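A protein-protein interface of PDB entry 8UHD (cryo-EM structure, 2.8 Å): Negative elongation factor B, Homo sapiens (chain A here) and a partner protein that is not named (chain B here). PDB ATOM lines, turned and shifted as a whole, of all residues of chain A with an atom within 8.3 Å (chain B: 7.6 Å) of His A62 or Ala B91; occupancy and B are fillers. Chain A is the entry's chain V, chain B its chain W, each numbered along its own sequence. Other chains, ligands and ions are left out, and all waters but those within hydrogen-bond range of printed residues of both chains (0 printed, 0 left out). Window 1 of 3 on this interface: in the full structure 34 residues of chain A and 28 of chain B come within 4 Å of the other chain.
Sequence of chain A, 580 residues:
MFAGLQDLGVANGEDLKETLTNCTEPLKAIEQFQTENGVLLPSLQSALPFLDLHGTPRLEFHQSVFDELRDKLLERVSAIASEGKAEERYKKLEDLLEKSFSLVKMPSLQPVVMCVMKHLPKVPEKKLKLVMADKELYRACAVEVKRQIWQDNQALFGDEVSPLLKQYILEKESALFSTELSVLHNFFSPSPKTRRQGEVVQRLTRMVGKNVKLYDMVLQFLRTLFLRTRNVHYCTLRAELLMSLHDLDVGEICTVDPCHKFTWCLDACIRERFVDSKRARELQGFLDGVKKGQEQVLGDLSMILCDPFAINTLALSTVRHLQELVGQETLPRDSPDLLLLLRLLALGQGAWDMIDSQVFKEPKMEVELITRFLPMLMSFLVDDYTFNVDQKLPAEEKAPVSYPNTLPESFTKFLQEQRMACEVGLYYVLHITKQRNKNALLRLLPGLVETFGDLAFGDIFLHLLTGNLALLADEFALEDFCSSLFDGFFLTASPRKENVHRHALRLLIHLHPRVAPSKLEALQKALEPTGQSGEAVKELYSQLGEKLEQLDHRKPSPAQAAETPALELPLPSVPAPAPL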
ATOM      1  N   GLN A  34       6.528   0.592   0.509  1.00  0.00           N
ATOM      2  CA  GLN A  34       6.687   0.049  -0.837  1.00  0.00           C
ATOM      3  C   GLN A  34       6.850  -1.465  -0.833  1.00  0.00           C
ATOM      4  O   GLN A  34       6.497  -2.124  -1.820  1.00  0.00           O
ATOM      5  CB  GLN A  34       7.882   0.703  -1.534  1.00  0.00           C
ATOM      6  CG  GLN A  34       7.673   2.168  -1.893  1.00  0.00           C
ATOM      7  CD  GLN A  34       8.772   2.718  -2.787  1.00  0.00           C
ATOM      8  OE1 GLN A  34       9.502   1.965  -3.432  1.00  0.00           O
ATOM      9  NE2 GLN A  34       8.883   4.040  -2.840  1.00  0.00           N
ATOM     10  N   ASN A  37       3.181  -2.826   0.457  1.00  0.00           N
ATOM     11  CA  ASN A  37       2.108  -2.356  -0.415  1.00  0.00           C
ATOM     12  C   ASN A  37       2.422  -2.647  -1.883  1.00  0.00           C
ATOM     13  O   ASN A  37       2.001  -1.905  -2.773  1.00  0.00           O
ATOM     14  CB  ASN A  37       1.844  -0.862  -0.207  1.00  0.00           C
ATOM     15  CG  ASN A  37       1.403  -0.527   1.216  1.00  0.00           C
ATOM     16  OD1 ASN A  37       0.240  -0.196   1.449  1.00  0.00           O
ATOM     17  ND2 ASN A  37       2.332  -0.583   2.167  1.00  0.00           N
ATOM     18  N   GLY A  38       3.162  -3.726  -2.146  1.00  0.00           N
ATOM     19  CA  GLY A  38       3.405  -4.210  -3.491  1.00  0.00           C
ATOM     20  C   GLY A  38       2.368  -5.229  -3.917  1.00  0.00           C
ATOM     21  O   GLY A  38       1.271  -5.307  -3.356  1.00  0.00           O
ATOM     22  N   VAL A  39       2.728  -6.028  -4.926  1.00  0.00           N
ATOM     23  CA  VAL A  39       1.810  -7.011  -5.501  1.00  0.00           C
ATOM     24  C   VAL A  39       2.061  -8.367  -4.846  1.00  0.00           C
ATOM     25  O   VAL A  39       3.211  -8.746  -4.592  1.00  0.00           O
ATOM     26  CB  VAL A  39       1.954  -7.074  -7.038  1.00  0.00           C
ATOM     27  CG1 VAL A  39       0.914  -8.028  -7.650  1.00  0.00           C
ATOM     28  CG2 VAL A  39       1.835  -5.671  -7.669  1.00  0.00           C
ATOM     29  N   LEU A  40       0.974  -9.088  -4.572  1.00  0.00           N
ATOM     30  CA  LEU A  40       0.949 -10.288  -3.727  1.00  0.00           C
ATOM     31  C   LEU A  40       1.129 -11.536  -4.593  1.00  0.00           C
ATOM     32  O   LEU A  40       0.161 -12.106  -5.097  1.00  0.00           O
ATOM     33  CB  LEU A  40      -0.368 -10.369  -2.953  1.00  0.00           C
ATOM     34  CG  LEU A  40      -0.844  -9.152  -2.153  1.00  0.00           C
ATOM     35  CD1 LEU A  40      -2.253  -9.374  -1.601  1.00  0.00           C
ATOM     36  CD2 LEU A  40       0.088  -8.811  -0.987  1.00  0.00           C
ATOM     37  N   LEU A  44       6.736 -12.053  -8.524  1.00  0.00           N
ATOM     38  CA  LEU A  44       6.963 -10.619  -8.612  1.00  0.00           C
ATOM     39  C   LEU A  44       7.938 -10.170  -7.533  1.00  0.00           C
ATOM     40  O   LEU A  44       8.818  -9.363  -7.800  1.00  0.00           O
ATOM     41  CB  LEU A  44       5.634  -9.894  -8.507  1.00  0.00           C
ATOM     42  CG  LEU A  44       4.557 -10.324  -9.519  1.00  0.00           C
ATOM     43  CD1 LEU A  44       3.288  -9.574  -9.225  1.00  0.00           C
ATOM     44  CD2 LEU A  44       4.967 -10.147 -10.983  1.00  0.00           C
ATOM     45  N   LEU A  48      10.513  -7.570  -8.986  1.00  0.00           N
ATOM     46  CA  LEU A  48      10.285  -6.129  -8.844  1.00  0.00           C
ATOM     47  C   LEU A  48      11.575  -5.324  -8.728  1.00  0.00           C
ATOM     48  O   LEU A  48      11.678  -4.282  -9.399  1.00  0.00           O
ATOM     49  CB  LEU A  48       9.340  -5.853  -7.662  1.00  0.00           C
ATOM     50  CG  LEU A  48       7.861  -6.267  -7.763  1.00  0.00           C
ATOM     51  CD1 LEU A  48       7.149  -5.991  -6.451  1.00  0.00           C
ATOM     52  CD2 LEU A  48       7.126  -5.590  -8.914  1.00  0.00           C
ATOM     53  N   LEU A  51      12.924  -5.629 -12.212  1.00  0.00           N
ATOM     54  CA  LEU A  51      12.047  -4.861 -13.090  1.00  0.00           C
ATOM     55  C   LEU A  51      12.372  -3.385 -12.998  1.00  0.00           C
ATOM     56  O   LEU A  51      12.428  -2.682 -14.014  1.00  0.00           O
ATOM     57  CB  LEU A  51      10.584  -5.108 -12.695  1.00  0.00           C
ATOM     58  CG  LEU A  51       9.423  -4.279 -13.281  1.00  0.00           C
ATOM     59  CD1 LEU A  51       9.096  -4.705 -14.702  1.00  0.00           C
ATOM     60  CD2 LEU A  51       8.190  -4.377 -12.388  1.00  0.00           C
ATOM     61  N   PRO A  57       9.700   2.677 -14.436  1.00  0.00           N
ATOM     62  CA  PRO A  57       8.811   2.928 -13.299  1.00  0.00           C
ATOM     63  C   PRO A  57       7.874   1.758 -13.074  1.00  0.00           C
ATOM     64  O   PRO A  57       7.468   1.065 -14.011  1.00  0.00           O
ATOM     65  CB  PRO A  57       8.034   4.186 -13.700  1.00  0.00           C
ATOM     66  CG  PRO A  57       8.292   4.415 -15.134  1.00  0.00           C
ATOM     67  CD  PRO A  57       9.215   3.365 -15.649  1.00  0.00           C
ATOM     68  N   ARG A  58       7.526   1.543 -11.806  1.00  0.00           N
ATOM     69  CA  ARG A  58       6.453   0.607 -11.506  1.00  0.00           C
ATOM     70  C   ARG A  58       5.094   1.132 -11.962  1.00  0.00           C
ATOM     71  O   ARG A  58       4.148   0.344 -12.036  1.00  0.00           O
ATOM     72  CB  ARG A  58       6.411   0.292 -10.009  1.00  0.00           C
ATOM     73  CG  ARG A  58       7.705  -0.280  -9.408  1.00  0.00           C
ATOM     74  CD  ARG A  58       7.545  -1.740  -8.977  1.00  0.00           C
ATOM     75  NE  ARG A  58       8.690  -2.227  -8.210  1.00  0.00           N
ATOM     76  CZ  ARG A  58       8.878  -2.050  -6.905  1.00  0.00           C
ATOM     77  NH1 ARG A  58       8.017  -1.375  -6.156  1.00  0.00           N
ATOM     78  NH2 ARG A  58       9.962  -2.567  -6.332  1.00  0.00           N
ATOM     79  N   LEU A  59       4.979   2.437 -12.256  1.00  0.00           N
ATOM     80  CA  LEU A  59       3.742   3.010 -12.791  1.00  0.00           C
ATOM     81  C   LEU A  59       3.271   2.268 -14.034  1.00  0.00           C
ATOM     82  O   LEU A  59       2.095   1.910 -14.145  1.00  0.00           O
ATOM     83  CB  LEU A  59       3.952   4.498 -13.116  1.00  0.00           C
ATOM     84  CG  LEU A  59       3.111   5.201 -14.207  1.00  0.00           C
ATOM     85  CD1 LEU A  59       1.624   5.221 -13.819  1.00  0.00           C
ATOM     86  CD2 LEU A  59       3.674   6.594 -14.492  1.00  0.00           C
ATOM     87  N   GLU A  60       4.172   2.082 -15.002  1.00  0.00           N
ATOM     88  CA  GLU A  60       3.792   1.469 -16.272  1.00  0.00           C
ATOM     89  C   GLU A  60       3.306   0.043 -16.055  1.00  0.00           C
ATOM     90  O   GLU A  60       2.273  -0.366 -16.602  1.00  0.00           O
ATOM     91  CB  GLU A  60       4.986   1.502 -17.229  1.00  0.00           C
ATOM     92  CG  GLU A  60       4.691   1.086 -18.674  1.00  0.00           C
ATOM     93  CD  GLU A  60       5.895   0.479 -19.378  1.00  0.00           C
ATOM     94  OE1 GLU A  60       7.040   0.699 -18.927  1.00  0.00           O
ATOM     95  OE2 GLU A  60       5.693  -0.225 -20.389  1.00  0.00           O
ATOM     96  N   PHE A  61       4.036  -0.719 -15.237  1.00  0.00           N
ATOM     97  CA  PHE A  61       3.637  -2.087 -14.920  1.00  0.00           C
ATOM     98  C   PHE A  61       2.269  -2.113 -14.252  1.00  0.00           C
ATOM     99  O   PHE A  61       1.373  -2.849 -14.688  1.00  0.00           O
ATOM    100  CB  PHE A  61       4.705  -2.736 -14.032  1.00  0.00           C
ATOM    101  CG  PHE A  61       4.202  -3.877 -13.190  1.00  0.00           C
ATOM    102  CD1 PHE A  61       3.741  -5.048 -13.772  1.00  0.00           C
ATOM    103  CD2 PHE A  61       4.218  -3.786 -11.809  1.00  0.00           C
ATOM    104  CE1 PHE A  61       3.286  -6.095 -12.989  1.00  0.00           C
ATOM    105  CE2 PHE A  61       3.765  -4.828 -11.022  1.00  0.00           C
ATOM    106  CZ  PHE A  61       3.301  -5.984 -11.612  1.00  0.00           C
ATOM    107  N   HIS A  62       2.085  -1.288 -13.211  1.00  0.00           N
ATOM    108  CA  HIS A  62       0.824  -1.260 -12.472  1.00  0.00           C
ATOM    109  C   HIS A  62      -0.337  -0.900 -13.387  1.00  0.00           C
ATOM    110  O   HIS A  62      -1.378  -1.562 -13.372  1.00  0.00           O
ATOM    111  CB  HIS A  62       0.895  -0.253 -11.318  1.00  0.00           C
ATOM    112  CG  HIS A  62       1.922  -0.571 -10.277  1.00  0.00           C
ATOM    113  ND1 HIS A  62       2.409  -1.842 -10.065  1.00  0.00           N
ATOM    114  CD2 HIS A  62       2.562   0.230  -9.392  1.00  0.00           C
ATOM    115  CE1 HIS A  62       3.304  -1.811  -9.092  1.00  0.00           C
ATOM    116  NE2 HIS A  62       3.411  -0.566  -8.664  1.00  0.00           N
ATOM    117  N   GLN A  63      -0.163   0.140 -14.206  1.00  0.00           N
ATOM    118  CA  GLN A  63      -1.226   0.584 -15.101  1.00  0.00           C
ATOM    119  C   GLN A  63      -1.577  -0.494 -16.118  1.00  0.00           C
ATOM    120  O   GLN A  63      -2.760  -0.756 -16.369  1.00  0.00           O
ATOM    121  CB  GLN A  63      -0.799   1.880 -15.799  1.00  0.00           C
ATOM    122  CG  GLN A  63      -1.658   2.316 -17.000  1.00  0.00           C
ATOM    123  CD  GLN A  63      -1.139   1.818 -18.347  1.00  0.00           C
ATOM    124  OE1 GLN A  63       0.067   1.677 -18.558  1.00  0.00           O
ATOM    125  NE2 GLN A  63      -2.060   1.544 -19.264  1.00  0.00           N
ATOM    126  N   SER A  64      -0.563  -1.135 -16.708  1.00  0.00           N
ATOM    127  CA  SER A  64      -0.824  -2.135 -17.739  1.00  0.00           C
ATOM    128  C   SER A  64      -1.574  -3.332 -17.168  1.00  0.00           C
ATOM    129  O   SER A  64      -2.596  -3.761 -17.723  1.00  0.00           O
ATOM    130  CB  SER A  64       0.493  -2.579 -18.377  1.00  0.00           C
ATOM    131  OG  SER A  64       1.337  -3.198 -17.422  1.00  0.00           O
ATOM    132  N   VAL A  65      -1.090  -3.881 -16.049  1.00  0.00           N
ATOM    133  CA  VAL A  65      -1.771  -5.051 -15.489  1.00  0.00           C
ATOM    134  C   VAL A  65      -3.135  -4.665 -14.924  1.00  0.00           C
ATOM    135  O   VAL A  65      -4.077  -5.466 -14.978  1.00  0.00           O
ATOM    136  CB  VAL A  65      -0.916  -5.798 -14.437  1.00  0.00           C
ATOM    137  CG1 VAL A  65       0.155  -6.633 -15.129  1.00  0.00           C
ATOM    138  CG2 VAL A  65      -0.280  -4.878 -13.397  1.00  0.00           C
ATOM    139  N   PHE A  66      -3.286  -3.440 -14.404  1.00  0.00           N
ATOM    140  CA  PHE A  66      -4.592  -2.990 -13.931  1.00  0.00           C
ATOM    141  C   PHE A  66      -5.595  -2.945 -15.075  1.00  0.00           C
ATOM    142  O   PHE A  66      -6.715  -3.450 -14.948  1.00  0.00           O
ATOM    143  CB  PHE A  66      -4.462  -1.615 -13.267  1.00  0.00           C
ATOM    144  CG  PHE A  66      -5.735  -0.808 -13.262  1.00  0.00           C
ATOM    145  CD1 PHE A  66      -6.850  -1.226 -12.551  1.00  0.00           C
ATOM    146  CD2 PHE A  66      -5.805   0.384 -13.965  1.00  0.00           C
ATOM    147  CE1 PHE A  66      -8.014  -0.474 -12.555  1.00  0.00           C
ATOM    148  CE2 PHE A  66      -6.963   1.139 -13.968  1.00  0.00           C
ATOM    149  CZ  PHE A  66      -8.067   0.710 -13.262  1.00  0.00           C
ATOM    150  N   ASP A  67      -5.200  -2.359 -16.208  1.00  0.00           N
ATOM    151  CA  ASP A  67      -6.099  -2.294 -17.356  1.00  0.00           C
ATOM    152  C   ASP A  67      -6.435  -3.688 -17.872  1.00  0.00           C
ATOM    153  O   ASP A  67      -7.601  -3.983 -18.164  1.00  0.00           O
ATOM    154  CB  ASP A  67      -5.474  -1.446 -18.464  1.00  0.00           C
ATOM    155  CG  ASP A  67      -5.182  -0.026 -18.017  1.00  0.00           C
ATOM    156  OD1 ASP A  67      -5.931   0.499 -17.166  1.00  0.00           O
ATOM    157  OD2 ASP A  67      -4.201   0.565 -18.516  1.00  0.00           O
ATOM    158  N   GLU A  68      -5.433  -4.569 -17.960  1.00  0.00           N
ATOM    159  CA  GLU A  68      -5.666  -5.912 -18.487  1.00  0.00           C
ATOM    160  C   GLU A  68      -6.624  -6.701 -17.597  1.00  0.00           C
ATOM    161  O   GLU A  68      -7.616  -7.273 -18.074  1.00  0.00           O
ATOM    162  CB  GLU A  68      -4.325  -6.642 -18.631  1.00  0.00           C
ATOM    163  CG  GLU A  68      -4.408  -8.117 -19.031  1.00  0.00           C
ATOM    164  CD  GLU A  68      -5.279  -8.359 -20.249  1.00  0.00           C
ATOM    165  OE1 GLU A  68      -5.316  -7.485 -21.141  1.00  0.00           O
ATOM    166  OE2 GLU A  68      -5.928  -9.423 -20.313  1.00  0.00           O
ATOM    167  N   LEU A  69      -6.359  -6.730 -16.292  1.00  0.00           N
ATOM    168  CA  LEU A  69      -7.202  -7.523 -15.408  1.00  0.00           C
ATOM    169  C   LEU A  69      -8.561  -6.866 -15.154  1.00  0.00           C
ATOM    170  O   LEU A  69      -9.530  -7.571 -14.854  1.00  0.00           O
ATOM    171  CB  LEU A  69      -6.453  -7.796 -14.103  1.00  0.00           C
ATOM    172  CG  LEU A  69      -5.447  -8.956 -14.072  1.00  0.00           C
ATOM    173  CD1 LEU A  69      -4.259  -8.747 -15.007  1.00  0.00           C
ATOM    174  CD2 LEU A  69      -4.953  -9.174 -12.648  1.00  0.00           C
ATOM    175  N   ASP B  55       1.624   7.792  -9.908  1.00  0.00           N
ATOM    176  CA  ASP B  55       2.410   6.756  -9.217  1.00  0.00           C
ATOM    177  C   ASP B  55       3.914   6.889  -9.450  1.00  0.00           C
ATOM    178  O   ASP B  55       4.640   5.891  -9.464  1.00  0.00           O
ATOM    179  CB  ASP B  55       1.955   5.351  -9.622  1.00  0.00           C
ATOM    180  CG  ASP B  55       0.475   5.137  -9.427  1.00  0.00           C
ATOM    181  OD1 ASP B  55      -0.224   6.092  -9.030  1.00  0.00           O
ATOM    182  OD2 ASP B  55       0.013   4.003  -9.667  1.00  0.00           O
ATOM    183  N   MET B  58       7.004   5.381  -6.978  1.00  0.00           N
ATOM    184  CA  MET B  58       7.665   4.083  -7.047  1.00  0.00           C
ATOM    185  C   MET B  58       8.909   4.073  -7.932  1.00  0.00           C
ATOM    186  O   MET B  58       9.642   3.078  -7.912  1.00  0.00           O
ATOM    187  CB  MET B  58       6.686   3.014  -7.550  1.00  0.00           C
ATOM    188  CG  MET B  58       5.415   2.834  -6.719  1.00  0.00           C
ATOM    189  SD  MET B  58       5.472   1.396  -5.635  1.00  0.00           S
ATOM    190  CE  MET B  58       4.591   2.032  -4.211  1.00  0.00           C
ATOM    191  N   TYR B  87      -0.813   9.494  -6.591  1.00  0.00           N
ATOM    192  CA  TYR B  87      -0.736   8.075  -6.268  1.00  0.00           C
ATOM    193  C   TYR B  87      -2.143   7.550  -6.018  1.00  0.00           C
ATOM    194  O   TYR B  87      -2.865   8.081  -5.166  1.00  0.00           O
ATOM    195  CB  TYR B  87       0.149   7.840  -5.045  1.00  0.00           C
ATOM    196  CG  TYR B  87       0.421   6.380  -4.764  1.00  0.00           C
ATOM    197  CD1 TYR B  87       1.285   5.652  -5.569  1.00  0.00           C
ATOM    198  CD2 TYR B  87      -0.179   5.734  -3.693  1.00  0.00           C
ATOM    199  CE1 TYR B  87       1.543   4.319  -5.320  1.00  0.00           C
ATOM    200  CE2 TYR B  87       0.072   4.398  -3.434  1.00  0.00           C
ATOM    201  CZ  TYR B  87       0.936   3.697  -4.251  1.00  0.00           C
ATOM    202  OH  TYR B  87       1.190   2.368  -4.000  1.00  0.00           O
ATOM    203  N   THR B  88      -2.523   6.508  -6.762  1.00  0.00           N
ATOM    204  CA  THR B  88      -3.838   5.880  -6.658  1.00  0.00           C
ATOM    205  C   THR B  88      -3.764   4.414  -6.246  1.00  0.00           C
ATOM    206  O   THR B  88      -4.794   3.728  -6.273  1.00  0.00           O
ATOM    207  CB  THR B  88      -4.591   6.005  -7.987  1.00  0.00           C
ATOM    208  OG1 THR B  88      -3.748   5.582  -9.066  1.00  0.00           O
ATOM    209  CG2 THR B  88      -5.024   7.442  -8.220  1.00  0.00           C
ATOM    210  N   ALA B  89      -2.585   3.915  -5.854  1.00  0.00           N
ATOM    211  CA  ALA B  89      -2.416   2.532  -5.405  1.00  0.00           C
ATOM    212  C   ALA B  89      -2.846   1.541  -6.487  1.00  0.00           C
ATOM    213  O   ALA B  89      -3.607   0.603  -6.243  1.00  0.00           O
ATOM    214  CB  ALA B  89      -3.175   2.288  -4.095  1.00  0.00           C
ATOM    215  N   VAL B  90      -2.345   1.763  -7.706  1.00  0.00           N
ATOM    216  CA  VAL B  90      -2.709   0.904  -8.829  1.00  0.00           C
ATOM    217  C   VAL B  90      -2.153  -0.499  -8.622  1.00  0.00           C
ATOM    218  O   VAL B  90      -2.738  -1.482  -9.095  1.00  0.00           O
ATOM    219  CB  VAL B  90      -2.237   1.522 -10.164  1.00  0.00           C
ATOM    220  CG1 VAL B  90      -2.670   0.663 -11.361  1.00  0.00           C
ATOM    221  CG2 VAL B  90      -2.794   2.932 -10.332  1.00  0.00           C
ATOM    222  N   ALA B  91      -1.015  -0.621  -7.932  1.00  0.00           N
ATOM    223  CA  ALA B  91      -0.513  -1.941  -7.563  1.00  0.00           C
ATOM    224  C   ALA B  91      -1.533  -2.687  -6.716  1.00  0.00           C
ATOM    225  O   ALA B  91      -1.884  -3.833  -7.014  1.00  0.00           O
ATOM    226  CB  ALA B  91       0.810  -1.817  -6.810  1.00  0.00           C
ATOM    227  N   GLN B  92      -2.057  -2.031  -5.679  1.00  0.00           N
ATOM    228  CA  GLN B  92      -3.046  -2.678  -4.821  1.00  0.00           C
ATOM    229  C   GLN B  92      -4.331  -2.957  -5.585  1.00  0.00           C
ATOM    230  O   GLN B  92      -5.026  -3.940  -5.294  1.00  0.00           O
ATOM    231  CB  GLN B  92      -3.343  -1.818  -3.588  1.00  0.00           C
ATOM    232  CG  GLN B  92      -2.165  -1.599  -2.630  1.00  0.00           C
ATOM    233  CD  GLN B  92      -1.223  -0.495  -3.085  1.00  0.00           C
ATOM    234  OE1 GLN B  92      -0.872  -0.414  -4.260  1.00  0.00           O
ATOM    235  NE2 GLN B  92      -0.853   0.388  -2.167  1.00  0.00           N
ATOM    236  N   THR B  93      -4.652  -2.113  -6.570  1.00  0.00           N
ATOM    237  CA  THR B  93      -5.754  -2.419  -7.473  1.00  0.00           C
ATOM    238  C   THR B  93      -5.516  -3.751  -8.171  1.00  0.00           C
ATOM    239  O   THR B  93      -6.391  -4.623  -8.159  1.00  0.00           O
ATOM    240  CB  THR B  93      -5.932  -1.295  -8.496  1.00  0.00           C
ATOM    241  OG1 THR B  93      -5.841  -0.025  -7.839  1.00  0.00           O
ATOM    242  CG2 THR B  93      -7.289  -1.406  -9.184  1.00  0.00           C
ATOM    243  N   VAL B  94      -4.315  -3.945  -8.733  1.00  0.00           N
ATOM    244  CA  VAL B  94      -3.989  -5.210  -9.401  1.00  0.00           C
ATOM    245  C   VAL B  94      -4.073  -6.364  -8.413  1.00  0.00           C
ATOM    246  O   VAL B  94      -4.442  -7.483  -8.783  1.00  0.00           O
ATOM    247  CB  VAL B  94      -2.593  -5.151 -10.069  1.00  0.00           C
ATOM    248  CG1 VAL B  94      -2.220  -6.507 -10.819  1.00  0.00           C
ATOM    249  CG2 VAL B  94      -2.466  -3.949 -11.054  1.00  0.00           C
ATOM    250  N   ASN B  95      -3.682  -6.130  -7.160  1.00  0.00           N
ATOM    251  CA  ASN B  95      -3.811  -7.180  -6.150  1.00  0.00           C
ATOM    252  C   ASN B  95      -5.265  -7.580  -5.973  1.00  0.00           C
ATOM    253  O   ASN B  95      -5.587  -8.773  -5.897  1.00  0.00           O
ATOM    254  CB  ASN B  95      -3.234  -6.727  -4.812  1.00  0.00           C
ATOM    255  CG  ASN B  95      -1.836  -6.213  -4.938  1.00  0.00           C
ATOM    256  OD1 ASN B  95      -1.301  -6.158  -6.036  1.00  0.00           O
ATOM    257  ND2 ASN B  95      -1.237  -5.813  -3.823  1.00  0.00           N
ATOM    258  N   LEU B  96      -6.155  -6.589  -5.914  1.00  0.00           N
ATOM    259  CA  LEU B  96      -7.581  -6.879  -5.801  1.00  0.00           C
ATOM    260  C   LEU B  96      -8.085  -7.640  -7.024  1.00  0.00           C
ATOM    261  O   LEU B  96      -8.887  -8.570  -6.898  1.00  0.00           O
ATOM    262  CB  LEU B  96      -8.372  -5.584  -5.592  1.00  0.00           C
ATOM    263  CG  LEU B  96      -8.611  -5.096  -4.148  1.00  0.00           C
ATOM    264  CD1 LEU B  96      -9.477  -6.071  -3.350  1.00  0.00           C
ATOM    265  CD2 LEU B  96      -7.312  -4.806  -3.389  1.00  0.00           C
ATOM    266  N   LEU B  97      -7.609  -7.276  -8.218  1.00  0.00           N
ATOM    267  CA  LEU B  97      -8.028  -8.005  -9.417  1.00  0.00           C
ATOM    268  C   LEU B  97      -7.500  -9.442  -9.416  1.00  0.00           C
ATOM    269  O   LEU B  97      -8.222 -10.374  -9.779  1.00  0.00           O
ATOM    270  CB  LEU B  97      -7.573  -7.286 -10.688  1.00  0.00           C
ATOM    271  CG  LEU B  97      -7.830  -5.786 -10.888  1.00  0.00           C
ATOM    272  CD1 LEU B  97      -7.024  -5.192 -12.037  1.00  0.00           C
ATOM    273  CD2 LEU B  97      -9.288  -5.513 -11.104  1.00  0.00           C
ATOM    274  N   ALA B  98      -6.245  -9.649  -9.031  1.00  0.00           N
ATOM    275  CA  ALA B  98      -5.684 -11.000  -9.051  1.00  0.00           C
ATOM    276  C   ALA B  98      -6.380 -11.893  -8.031  1.00  0.00           C
ATOM    277  O   ALA B  98      -6.720 -13.048  -8.327  1.00  0.00           O
ATOM    278  CB  ALA B  98      -4.179 -10.948  -8.795  1.00  0.00           C
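SD of Met B58 is in hydrogen-bond range of NH1 of Arg A58 (3.8 Å).
The side-chain amide nitrogen (ND2) of Asn B95 sits at hydrogen-bond distance from the backbone carbonyl oxygen (O) of Gly A38, at 2.6 Å.
N of Thr B88 sits at hydrogen-bond distance from OD1 of Asp B55 (3.3 Å).
OH of Tyr B87 lies within hydrogen-bond range of NE2 of Gln B92 (3.4 Å).
The side-chain hydroxyl (OG1) of Thr B93 lies within hydrogen-bond range of the backbone carbonyl oxygen (O) of Ala B89.
The backbone carbonyl oxygen (O) of Ala B91 sits close to the side-chain amide oxygen (OD1) of Asn B95 (2.6 Å).
A ring nitrogen (ND1) of His A62 sits close to the backbone carbonyl oxygen (O) of Arg A58 (3.4 Å).
The side-chain amide nitrogen of Gln A63 is in hydrogen-bond range of the side-chain carboxylate of Asp A67 (2.5 Å).
Among the printed residues, pairs that only touch across the chains: His A62 with Val B90, Val A39 with Asn B95, Val A65 with Val B94, Leu A69 with Leu B97, His A62 with Ala B91, Phe A66 with Thr B93, Phe A66 with Leu B97, Phe A66 with Val B90, Phe A66 with Val B94, His A62 with Val B94, Asn A37 with Gln B92, Leu A40 with Asn B95, Gln A63 with Val B90, Gln A34 with Met B58, Leu A69 with Ala B98 and Leu A59 with Asp B55.
Of the printed residues of chain B, Asn A37 touches Gln B92.
Of the printed residues of chain B, Val A39 touches Asn B95.
Printed residues of chain B within 4 Å of Leu A40: Asn B95 (3.8 Å).
His A62 touches just these residues of chain B: Val B90, Ala B91 and Val B94.
Of the printed residues of chain A, Met B58 touches Gln A34 and Arg A58.
Of chain A, only His A62 (3.4 Å) comes within 4 Å of Ala B91.
Of the printed residues of chain A, Gln B92 touches Asn A37.
The nearest residue of chain A that does not touch Ala B91 is Val A39 (4.1 Å).
The nearest printed residue of chain B that does not touch Gly A38 is Ala B91 (4.7 Å).
Printed residues of chain B that touch a printed residue of chain A: Asp B55, Met B58, Val B90, Ala B91, Gln B92, Thr B93, Val B94, Asn B95, Leu B97 and Ala B98.
Hydrophobic or aromatic side chains of chain B that line the printed part of chain A: Met B58, Val B90, Ala B91, Val B94 and Leu B97.
Of the 21 printed residues of chain A, 12 touch a printed residue of chain B.
Printed residues of chain A that touch a printed residue of chain B: Gln A34, Asn A37, Gly A38, Val A39, Leu A40, Arg A58, Leu A59, His A62, Gln A63, Val A65, Phe A66 and Leu A69.
Among the printed residues, no Asp or Glu carboxylate lies within 4 Å of a Lys or Arg side-chain nitrogen of the other chain.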
